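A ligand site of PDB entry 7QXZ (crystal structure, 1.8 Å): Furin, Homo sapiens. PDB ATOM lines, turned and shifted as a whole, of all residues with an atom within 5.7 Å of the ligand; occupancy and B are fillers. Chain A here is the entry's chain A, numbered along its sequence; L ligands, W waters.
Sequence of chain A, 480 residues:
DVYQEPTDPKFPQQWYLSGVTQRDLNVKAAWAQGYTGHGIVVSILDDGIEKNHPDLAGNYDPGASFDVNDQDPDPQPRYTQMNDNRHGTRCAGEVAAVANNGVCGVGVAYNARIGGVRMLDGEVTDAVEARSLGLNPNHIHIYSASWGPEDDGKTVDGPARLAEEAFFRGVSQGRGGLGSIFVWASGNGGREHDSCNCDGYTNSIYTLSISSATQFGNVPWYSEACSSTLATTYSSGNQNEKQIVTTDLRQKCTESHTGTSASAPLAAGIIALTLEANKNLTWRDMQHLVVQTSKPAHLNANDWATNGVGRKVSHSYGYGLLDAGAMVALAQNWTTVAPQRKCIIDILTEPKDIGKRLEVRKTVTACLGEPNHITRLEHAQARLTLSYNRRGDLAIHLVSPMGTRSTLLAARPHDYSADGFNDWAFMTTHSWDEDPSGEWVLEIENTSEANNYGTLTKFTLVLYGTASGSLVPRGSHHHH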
ATOM      1  N   LEU A  45     -27.061  -3.967  24.445  1.00  0.00           N
ATOM      2  CA  LEU A  45     -25.791  -3.409  24.929  1.00  0.00           C
ATOM      3  C   LEU A  45     -25.949  -3.214  26.423  1.00  0.00           C
ATOM      4  O   LEU A  45     -26.672  -2.313  26.835  1.00  0.00           O
ATOM      5  CB  LEU A  45     -25.479  -2.054  24.237  1.00  0.00           C
ATOM      6  CG  LEU A  45     -25.541  -2.005  22.702  1.00  0.00           C
ATOM      7  CD1 LEU A  45     -24.904  -0.723  22.174  1.00  0.00           C
ATOM      8  CD2 LEU A  45     -24.850  -3.192  22.057  1.00  0.00           C
ATOM      9  N   ASP A  46     -25.333  -4.074  27.246  1.00  0.00           N
ATOM     10  CA  ASP A  46     -25.549  -4.000  28.689  1.00  0.00           C
ATOM     11  C   ASP A  46     -24.441  -4.736  29.463  1.00  0.00           C
ATOM     12  O   ASP A  46     -23.275  -4.673  29.049  1.00  0.00           O
ATOM     13  CB  ASP A  46     -27.001  -4.507  28.966  1.00  0.00           C
ATOM     14  CG  ASP A  46     -27.671  -3.912  30.187  1.00  0.00           C
ATOM     15  OD1 ASP A  46     -27.076  -3.971  31.274  1.00  0.00           O
ATOM     16  OD2 ASP A  46     -28.828  -3.415  30.056  1.00  0.00           O
ATOM     17  N   ASP A  47     -24.762  -5.404  30.587  1.00  0.00           N
ATOM     18  CA  ASP A  47     -23.820  -6.104  31.446  1.00  0.00           C
ATOM     19  C   ASP A  47     -23.650  -7.598  31.132  1.00  0.00           C
ATOM     20  O   ASP A  47     -23.092  -8.314  31.942  1.00  0.00           O
ATOM     21  CB  ASP A  47     -24.231  -5.916  32.919  1.00  0.00           C
ATOM     22  CG  ASP A  47     -25.679  -6.291  33.247  1.00  0.00           C
ATOM     23  OD1 ASP A  47     -26.282  -7.095  32.489  1.00  0.00           O
ATOM     24  OD2 ASP A  47     -26.214  -5.751  34.255  1.00  0.00           O
ATOM     25  N   ASP A  84     -25.650  -8.506  40.534  1.00  0.00           N
ATOM     26  CA  ASP A  84     -25.508  -7.175  39.948  1.00  0.00           C
ATOM     27  C   ASP A  84     -25.634  -7.163  38.416  1.00  0.00           C
ATOM     28  O   ASP A  84     -26.214  -6.216  37.871  1.00  0.00           O
ATOM     29  CB  ASP A  84     -24.155  -6.562  40.359  1.00  0.00           C
ATOM     30  CG  ASP A  84     -23.990  -6.337  41.856  1.00  0.00           C
ATOM     31  N   MET A 119     -20.648  -4.971  27.912  1.00  0.00           N
ATOM     32  CA  MET A 119     -19.866  -3.743  27.837  1.00  0.00           C
ATOM     33  C   MET A 119     -19.992  -2.823  29.078  1.00  0.00           C
ATOM     34  O   MET A 119     -19.167  -1.929  29.211  1.00  0.00           O
ATOM     35  CB  MET A 119     -20.290  -2.941  26.617  1.00  0.00           C
ATOM     36  CG  MET A 119     -21.779  -2.556  26.702  1.00  0.00           C
ATOM     37  SD  MET A 119     -22.341  -1.190  25.747  1.00  0.00           S
ATOM     38  CE  MET A 119     -21.016   0.066  26.015  1.00  0.00           C
ATOM     39  N   LEU A 120     -21.015  -2.992  29.942  1.00  0.00           N
ATOM     40  CA  LEU A 120     -21.138  -2.133  31.140  1.00  0.00           C
ATOM     41  C   LEU A 120     -20.450  -2.721  32.399  1.00  0.00           C
ATOM     42  O   LEU A 120     -20.441  -2.042  33.438  1.00  0.00           O
ATOM     43  CB  LEU A 120     -22.606  -1.819  31.448  1.00  0.00           C
ATOM     44  CG  LEU A 120     -23.412  -1.131  30.335  1.00  0.00           C
ATOM     45  CD1 LEU A 120     -24.843  -0.886  30.791  1.00  0.00           C
ATOM     46  CD2 LEU A 120     -22.767   0.197  29.913  1.00  0.00           C
ATOM     47  N   VAL A 124     -16.442   2.066  31.106  1.00  0.00           N
ATOM     48  CA  VAL A 124     -17.092   2.358  29.827  1.00  0.00           C
ATOM     49  C   VAL A 124     -16.362   3.523  29.177  1.00  0.00           C
ATOM     50  O   VAL A 124     -16.589   4.683  29.498  1.00  0.00           O
ATOM     51  CB  VAL A 124     -18.607   2.610  29.983  1.00  0.00           C
ATOM     52  CG1 VAL A 124     -19.256   2.868  28.614  1.00  0.00           C
ATOM     53  CG2 VAL A 124     -19.274   1.432  30.697  1.00  0.00           C
ATOM     54  N   THR A 125     -15.427   3.196  28.288  1.00  0.00           N
ATOM     55  CA  THR A 125     -14.640   4.167  27.556  1.00  0.00           C
ATOM     56  C   THR A 125     -15.243   4.365  26.172  1.00  0.00           C
ATOM     57  O   THR A 125     -16.077   3.564  25.733  1.00  0.00           O
ATOM     58  CB  THR A 125     -13.168   3.654  27.437  1.00  0.00           C
ATOM     59  OG1 THR A 125     -13.146   2.536  26.537  1.00  0.00           O
ATOM     60  CG2 THR A 125     -12.563   3.274  28.772  1.00  0.00           C
ATOM     61  N   ASP A 126     -14.788   5.409  25.466  1.00  0.00           N
ATOM     62  CA  ASP A 126     -15.183   5.719  24.110  1.00  0.00           C
ATOM     63  C   ASP A 126     -14.887   4.529  23.172  1.00  0.00           C
ATOM     64  O   ASP A 126     -15.725   4.187  22.351  1.00  0.00           O
ATOM     65  CB  ASP A 126     -14.447   6.993  23.645  1.00  0.00           C
ATOM     66  CG  ASP A 126     -14.805   7.495  22.279  1.00  0.00           C
ATOM     67  OD1 ASP A 126     -15.994   7.368  21.881  1.00  0.00           O
ATOM     68  OD2 ASP A 126     -13.904   8.052  21.609  1.00  0.00           O
ATOM     69  N   GLU A 129     -17.443   1.714  23.798  1.00  0.00           N
ATOM     70  CA  GLU A 129     -18.737   2.048  23.174  1.00  0.00           C
ATOM     71  C   GLU A 129     -18.696   1.842  21.670  1.00  0.00           C
ATOM     72  O   GLU A 129     -19.643   1.318  21.113  1.00  0.00           O
ATOM     73  CB  GLU A 129     -19.103   3.494  23.445  1.00  0.00           C
ATOM     74  CG  GLU A 129     -19.369   3.761  24.907  1.00  0.00           C
ATOM     75  CD  GLU A 129     -19.486   5.229  25.234  1.00  0.00           C
ATOM     76  OE1 GLU A 129     -19.737   6.039  24.307  1.00  0.00           O
ATOM     77  OE2 GLU A 129     -19.326   5.572  26.423  1.00  0.00           O
ATOM     78  N   SER A 132     -18.842  -1.776  20.690  1.00  0.00           N
ATOM     79  CA  SER A 132     -20.156  -2.317  20.974  1.00  0.00           C
ATOM     80  C   SER A 132     -21.157  -1.858  19.914  1.00  0.00           C
ATOM     81  O   SER A 132     -21.811  -2.695  19.297  1.00  0.00           O
ATOM     82  CB  SER A 132     -20.608  -1.892  22.376  1.00  0.00           C
ATOM     83  OG  SER A 132     -19.616  -2.255  23.310  1.00  0.00           O
ATOM     84  N   LEU A 133     -21.242  -0.536  19.665  1.00  0.00           N
ATOM     85  CA  LEU A 133     -22.129   0.032  18.656  1.00  0.00           C
ATOM     86  C   LEU A 133     -21.784  -0.498  17.243  1.00  0.00           C
ATOM     87  O   LEU A 133     -22.678  -0.679  16.430  1.00  0.00           O
ATOM     88  CB  LEU A 133     -22.057   1.581  18.677  1.00  0.00           C
ATOM     89  CG  LEU A 133     -22.565   2.272  19.961  1.00  0.00           C
ATOM     90  CD1 LEU A 133     -22.072   3.722  20.043  1.00  0.00           C
ATOM     91  CD2 LEU A 133     -24.082   2.243  20.057  1.00  0.00           C
ATOM     92  N   ALA A 145     -30.088  -0.157  23.702  1.00  0.00           N
ATOM     93  CA  ALA A 145     -29.253   0.362  24.774  1.00  0.00           C
ATOM     94  C   ALA A 145     -30.170   1.053  25.765  1.00  0.00           C
ATOM     95  O   ALA A 145     -30.927   1.941  25.410  1.00  0.00           O
ATOM     96  CB  ALA A 145     -28.236   1.339  24.202  1.00  0.00           C
ATOM     97  N   SER A 146     -30.091   0.635  27.007  1.00  0.00           N
ATOM     98  CA  SER A 146     -30.955   1.117  28.073  1.00  0.00           C
ATOM     99  C   SER A 146     -30.331   2.146  28.986  1.00  0.00           C
ATOM    100  O   SER A 146     -31.020   2.634  29.877  1.00  0.00           O
ATOM    101  CB  SER A 146     -31.410  -0.078  28.914  1.00  0.00           C
ATOM    102  OG  SER A 146     -32.434  -0.820  28.276  1.00  0.00           O
ATOM    103  N   TRP A 147     -29.047   2.493  28.793  1.00  0.00           N
ATOM    104  CA  TRP A 147     -28.346   3.399  29.701  1.00  0.00           C
ATOM    105  C   TRP A 147     -27.471   4.377  28.933  1.00  0.00           C
ATOM    106  O   TRP A 147     -27.345   4.290  27.712  1.00  0.00           O
ATOM    107  CB  TRP A 147     -27.477   2.545  30.673  1.00  0.00           C
ATOM    108  CG  TRP A 147     -28.161   1.355  31.255  1.00  0.00           C
ATOM    109  CD1 TRP A 147     -28.156   0.087  30.762  1.00  0.00           C
ATOM    110  CD2 TRP A 147     -29.021   1.332  32.405  1.00  0.00           C
ATOM    111  NE1 TRP A 147     -28.880  -0.746  31.585  1.00  0.00           N
ATOM    112  CE2 TRP A 147     -29.421  -0.004  32.600  1.00  0.00           C
ATOM    113  CE3 TRP A 147     -29.401   2.305  33.344  1.00  0.00           C
ATOM    114  CZ2 TRP A 147     -30.234  -0.390  33.666  1.00  0.00           C
ATOM    115  CZ3 TRP A 147     -30.187   1.914  34.409  1.00  0.00           C
ATOM    116  CH2 TRP A 147     -30.592   0.589  34.569  1.00  0.00           C
ATOM    117  N   GLY A 148     -26.879   5.310  29.655  1.00  0.00           N
ATOM    118  CA  GLY A 148     -25.990   6.294  29.060  1.00  0.00           C
ATOM    119  C   GLY A 148     -25.268   7.088  30.124  1.00  0.00           C
ATOM    120  O   GLY A 148     -25.030   6.552  31.210  1.00  0.00           O
ATOM    121  N   PRO A 149     -24.976   8.385  29.903  1.00  0.00           N
ATOM    122  CA  PRO A 149     -24.316   9.158  30.975  1.00  0.00           C
ATOM    123  C   PRO A 149     -25.178   9.312  32.231  1.00  0.00           C
ATOM    124  O   PRO A 149     -26.391   9.105  32.196  1.00  0.00           O
ATOM    125  CB  PRO A 149     -24.004  10.507  30.305  1.00  0.00           C
ATOM    126  CG  PRO A 149     -24.936  10.612  29.194  1.00  0.00           C
ATOM    127  CD  PRO A 149     -25.236   9.216  28.727  1.00  0.00           C
ATOM    128  N   GLU A 150     -24.517   9.638  33.344  1.00  0.00           N
ATOM    129  CA  GLU A 150     -25.168   9.696  34.645  1.00  0.00           C
ATOM    130  C   GLU A 150     -26.449  10.526  34.688  1.00  0.00           C
ATOM    131  O   GLU A 150     -26.464  11.684  34.285  1.00  0.00           O
ATOM    132  CB  GLU A 150     -24.183  10.169  35.713  1.00  0.00           C
ATOM    133  CG  GLU A 150     -24.767  10.052  37.104  1.00  0.00           C
ATOM    134  CD  GLU A 150     -23.798   9.728  38.227  1.00  0.00           C
ATOM    135  OE1 GLU A 150     -22.569   9.785  37.998  1.00  0.00           O
ATOM    136  OE2 GLU A 150     -24.286   9.429  39.349  1.00  0.00           O
ATOM    137  N   ASP A 157     -23.357  15.248  28.609  1.00  0.00           N
ATOM    138  CA  ASP A 157     -22.359  14.387  27.991  1.00  0.00           C
ATOM    139  C   ASP A 157     -22.970  13.569  26.876  1.00  0.00           C
ATOM    140  O   ASP A 157     -24.139  13.216  26.912  1.00  0.00           O
ATOM    141  CB  ASP A 157     -21.751  13.454  29.061  1.00  0.00           C
ATOM    142  CG  ASP A 157     -20.481  12.743  28.630  1.00  0.00           C
ATOM    143  OD1 ASP A 157     -19.764  13.270  27.748  1.00  0.00           O
ATOM    144  OD2 ASP A 157     -20.191  11.672  29.177  1.00  0.00           O
ATOM    145  N   GLY A 158     -22.145  13.266  25.893  1.00  0.00           N
ATOM    146  CA  GLY A 158     -22.560  12.528  24.715  1.00  0.00           C
ATOM    147  C   GLY A 158     -21.463  11.660  24.177  1.00  0.00           C
ATOM    148  O   GLY A 158     -20.385  11.557  24.761  1.00  0.00           O
ATOM    149  N   PRO A 159     -21.731  10.984  23.047  1.00  0.00           N
ATOM    150  CA  PRO A 159     -20.707  10.112  22.470  1.00  0.00           C
ATOM    151  C   PRO A 159     -19.467  10.898  22.069  1.00  0.00           C
ATOM    152  O   PRO A 159     -19.574  11.904  21.374  1.00  0.00           O
ATOM    153  CB  PRO A 159     -21.382   9.483  21.252  1.00  0.00           C
ATOM    154  CG  PRO A 159     -22.594  10.292  20.995  1.00  0.00           C
ATOM    155  CD  PRO A 159     -22.983  10.965  22.268  1.00  0.00           C
ATOM    156  N   ALA A 160     -18.303  10.449  22.503  1.00  0.00           N
ATOM    157  CA  ALA A 160     -17.029  11.037  22.107  1.00  0.00           C
ATOM    158  C   ALA A 160     -16.718  10.552  20.628  1.00  0.00           C
ATOM    159  O   ALA A 160     -17.582   9.933  19.989  1.00  0.00           O
ATOM    160  CB  ALA A 160     -15.939  10.667  23.121  1.00  0.00           C
ATOM    161  N   PHE A 167     -21.711   5.410  15.308  1.00  0.00           N
ATOM    162  CA  PHE A 167     -23.096   5.725  14.928  1.00  0.00           C
ATOM    163  C   PHE A 167     -23.167   6.104  13.445  1.00  0.00           C
ATOM    164  O   PHE A 167     -24.051   5.601  12.737  1.00  0.00           O
ATOM    165  CB  PHE A 167     -23.655   6.893  15.759  1.00  0.00           C
ATOM    166  CG  PHE A 167     -24.120   6.533  17.151  1.00  0.00           C
ATOM    167  CD1 PHE A 167     -25.139   5.610  17.338  1.00  0.00           C
ATOM    168  CD2 PHE A 167     -23.641   7.221  18.251  1.00  0.00           C
ATOM    169  CE1 PHE A 167     -25.603   5.327  18.616  1.00  0.00           C
ATOM    170  CE2 PHE A 167     -24.114   6.928  19.529  1.00  0.00           C
ATOM    171  CZ  PHE A 167     -25.106   5.999  19.699  1.00  0.00           C
ATOM    172  N   TRP A 184     -32.826   3.552  21.968  1.00  0.00           N
ATOM    173  CA  TRP A 184     -32.274   4.064  23.221  1.00  0.00           C
ATOM    174  C   TRP A 184     -33.337   4.444  24.241  1.00  0.00           C
ATOM    175  O   TRP A 184     -34.382   4.999  23.887  1.00  0.00           O
ATOM    176  CB  TRP A 184     -31.396   5.301  22.954  1.00  0.00           C
ATOM    177  CG  TRP A 184     -30.098   5.298  23.700  1.00  0.00           C
ATOM    178  CD1 TRP A 184     -29.886   5.685  24.990  1.00  0.00           C
ATOM    179  CD2 TRP A 184     -28.845   4.795  23.217  1.00  0.00           C
ATOM    180  NE1 TRP A 184     -28.570   5.465  25.342  1.00  0.00           N
ATOM    181  CE2 TRP A 184     -27.920   4.880  24.289  1.00  0.00           C
ATOM    182  CE3 TRP A 184     -28.423   4.257  22.006  1.00  0.00           C
ATOM    183  CZ2 TRP A 184     -26.598   4.487  24.153  1.00  0.00           C
ATOM    184  CZ3 TRP A 184     -27.107   3.869  21.876  1.00  0.00           C
ATOM    185  CH2 TRP A 184     -26.210   3.960  22.948  1.00  0.00           C
ATOM    186  N   TYR A 201     -26.577  10.580  23.677  1.00  0.00           N
ATOM    187  CA  TYR A 201     -26.924   9.309  23.047  1.00  0.00           C
ATOM    188  C   TYR A 201     -28.395   9.324  22.678  1.00  0.00           C
ATOM    189  O   TYR A 201     -28.737   9.086  21.524  1.00  0.00           O
ATOM    190  CB  TYR A 201     -26.602   8.120  23.970  1.00  0.00           C
ATOM    191  CG  TYR A 201     -25.140   8.054  24.308  1.00  0.00           C
ATOM    192  CD1 TYR A 201     -24.579   8.906  25.260  1.00  0.00           C
ATOM    193  CD2 TYR A 201     -24.272   7.225  23.602  1.00  0.00           C
ATOM    194  CE1 TYR A 201     -23.223   8.891  25.537  1.00  0.00           C
ATOM    195  CE2 TYR A 201     -22.924   7.171  23.893  1.00  0.00           C
ATOM    196  CZ  TYR A 201     -22.404   7.995  24.881  1.00  0.00           C
ATOM    197  OH  TYR A 201     -21.070   8.053  25.131  1.00  0.00           O
HETATM  198  N1  LIG L   1     -22.655   4.359  29.627  1.00  0.00           N
HETATM  199  C1  LIG L   1     -21.631   6.838  28.905  1.00  0.00           C
HETATM  200  C2  LIG L   1     -22.175   6.000  27.958  1.00  0.00           C
HETATM  201  C3  LIG L   1     -22.719   4.781  28.362  1.00  0.00           C
HETATM  202  C4  LIG L   1     -23.305   3.836  27.368  1.00  0.00           C
HETATM  203  C5  LIG L   1     -22.818   3.789  26.073  1.00  0.00           C
HETATM  204  C6  LIG L   1     -24.275   1.950  25.549  1.00  0.00           C
HETATM  205  C7  LIG L   1     -20.996   8.118  28.504  1.00  0.00           C
HETATM  206  C8  LIG L   1     -23.995   1.706  33.458  1.00  0.00           C
HETATM  207  C9  LIG L   1     -24.657  -0.521  36.177  1.00  0.00           C
HETATM  208  C10 LIG L   1     -26.743   0.370  35.278  1.00  0.00           C
HETATM  209  C11 LIG L   1     -24.722   1.981  26.850  1.00  0.00           C
HETATM  210  C12 LIG L   1     -24.263   2.901  27.764  1.00  0.00           C
HETATM  211  C13 LIG L   1     -22.705   3.756  32.365  1.00  0.00           C
HETATM  212  C14 LIG L   1     -24.068   3.628  32.263  1.00  0.00           C
HETATM  213  C15 LIG L   1     -22.088   5.166  30.523  1.00  0.00           C
HETATM  214  C16 LIG L   1     -22.044   2.786  33.079  1.00  0.00           C
HETATM  215  C17 LIG L   1     -24.004  -0.378  34.819  1.00  0.00           C
HETATM  216  C18 LIG L   1     -26.120   0.502  33.915  1.00  0.00           C
HETATM  217  C19 LIG L   1     -21.556   6.400  30.218  1.00  0.00           C
HETATM  218  C20 LIG L   1     -26.797  -0.989  37.334  1.00  0.00           C
HETATM  219  C21 LIG L   1     -18.966   9.104  27.348  1.00  0.00           C
HETATM  220  C22 LIG L   1     -17.504   8.614  27.159  1.00  0.00           C
HETATM  221  C23 LIG L   1     -17.273   7.588  28.248  1.00  0.00           C
HETATM  222  C24 LIG L   1     -18.615   7.442  28.950  1.00  0.00           C
HETATM  223  C25 LIG L   1     -15.250   9.404  27.105  1.00  0.00           C
HETATM  224  C26 LIG L   1     -14.536  10.525  26.429  1.00  0.00           C
HETATM  225  C27 LIG L   1     -23.319   2.871  25.183  1.00  0.00           C
HETATM  226  N2  LIG L   1     -19.622   7.909  27.947  1.00  0.00           N
HETATM  227  N3  LIG L   1     -24.734   2.607  32.801  1.00  0.00           N
HETATM  228  N4  LIG L   1     -22.673   1.733  33.618  1.00  0.00           N
HETATM  229  N5  LIG L   1     -24.663   0.671  34.026  1.00  0.00           N
HETATM  230  N6  LIG L   1     -26.128  -0.764  36.018  1.00  0.00           N
HETATM  231  O1  LIG L   1     -22.001   4.829  31.836  1.00  0.00           O
HETATM  232  O2  LIG L   1     -16.621   9.697  27.380  1.00  0.00           O
HETATM  233  O3  LIG L   1     -13.578  10.167  25.669  1.00  0.00           O
HETATM  234  O4  LIG L   1     -14.922  11.714  26.651  1.00  0.00           O
HETATM  235 CL1  LIG L   1     -25.935   0.842  27.351  1.00  0.00          CL
HETATM  236 CL2  LIG L   1     -22.731   2.857  23.550  1.00  0.00          CL
HETATM  237  O   HOH W   1     -12.796   7.170  26.796  1.00  0.00           O
HETATM  238  O   HOH W   2     -26.532  -2.937  33.980  1.00  0.00           O
HETATM  239  O   HOH W   3     -20.251   0.379  34.459  1.00  0.00           O
HETATM  240  O   HOH W   4     -23.784   6.628  33.848  1.00  0.00           O
HETATM  241  O   HOH W   5     -17.956  12.092  25.854  1.00  0.00           O
HETATM  242  O   HOH W   6     -16.965  10.868  29.863  1.00  0.00           O
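Water W6 bridges an oxygen (O2) of the ligand and the side-chain carboxylate (OD2) of Asp 157. Water W3 lies within hydrogen-bond range of O of Leu 120 (2.6 Å) and N4 of the ligand (2.9 Å). Water W2 lies within hydrogen-bond range of OD2 of Asp 47 (2.8 Å), OD1 of Asp 46 (2.9 Å) and N6 of the ligand (3.0 Å). Water W4 lies within hydrogen-bond range of O of Gly 148, N of Glu 150 and O1 of the ligand. Water W1 bridges the backbone NH (N) of Asp 126 (3.0 Å) and an oxygen (O3) of the ligand (3.3 Å).
O of Leu 45 touches CL1 of the ligand (3.3 Å). Met 119 touches the ligand (SD to C6, 3.7 Å). Leu 120 touches the ligand (CD1 to N5, 3.6 Å). Val 124 touches the ligand. CB of Asp 126 touches O3 of the ligand, 3.9 Å away. Leu 133 touches the ligand (CG to CL2, 3.6 Å). CB of Ala 145 touches CL1 of the ligand, 3.9 Å away. CD2 of Trp 147 touches C18 of the ligand, 3.4 Å away. Gly 148 touches the ligand (O to C14, 3.3 Å). Pro 149 touches the ligand. Asp 157 touches the ligand. Gly 158 touches the ligand (O to C21, 3.8 Å). Ala 160 touches the ligand. Trp 184 touches the ligand (CH2 to CL2, 3.7 Å). Hydrophobic or aromatic side chains within 4 Å of the ligand: Met 119, Leu 120, Val 124, Leu 133, Ala 145, Trp 147, Ala 160, Trp 184 and Tyr 201. Within 4 Å of the ligand: Leu 45, Met 119, Leu 120, Val 124, Asp 126, Glu 129, Leu 133, Ala 145, Trp 147, Gly 148, Pro 149, Asp 157, Gly 158, Ala 160, Trp 184 and Tyr 201. The nearest printed residue that does not touch the ligand is Ser 146 (4.2 Å).
O of Asp 46 sits at hydrogen-bond distance from N of Met 119 (2.9 Å). OE1 of Glu 129 sits at hydrogen-bond distance from OH of Tyr 201 (2.6 Å). The indole nitrogen (NE1) of Trp 147 is in hydrogen-bond range of the side-chain carboxylate (OD2) of Asp 46. O of Asp 46 lies within hydrogen-bond range of N of Leu 120 (3.0 Å). The indole nitrogen (NE1) of Trp 184 is in hydrogen-bond range of the backbone carbonyl oxygen (O) of Trp 147 (2.9 Å).
N2 of the ligand sits at hydrogen-bond distance from OH of Tyr 201, 3.2 Å away. The side-chain carboxylate (OE2) of Glu 129 is in salt-bridge range of a nitrogen (N2) of the ligand (2.8 Å).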
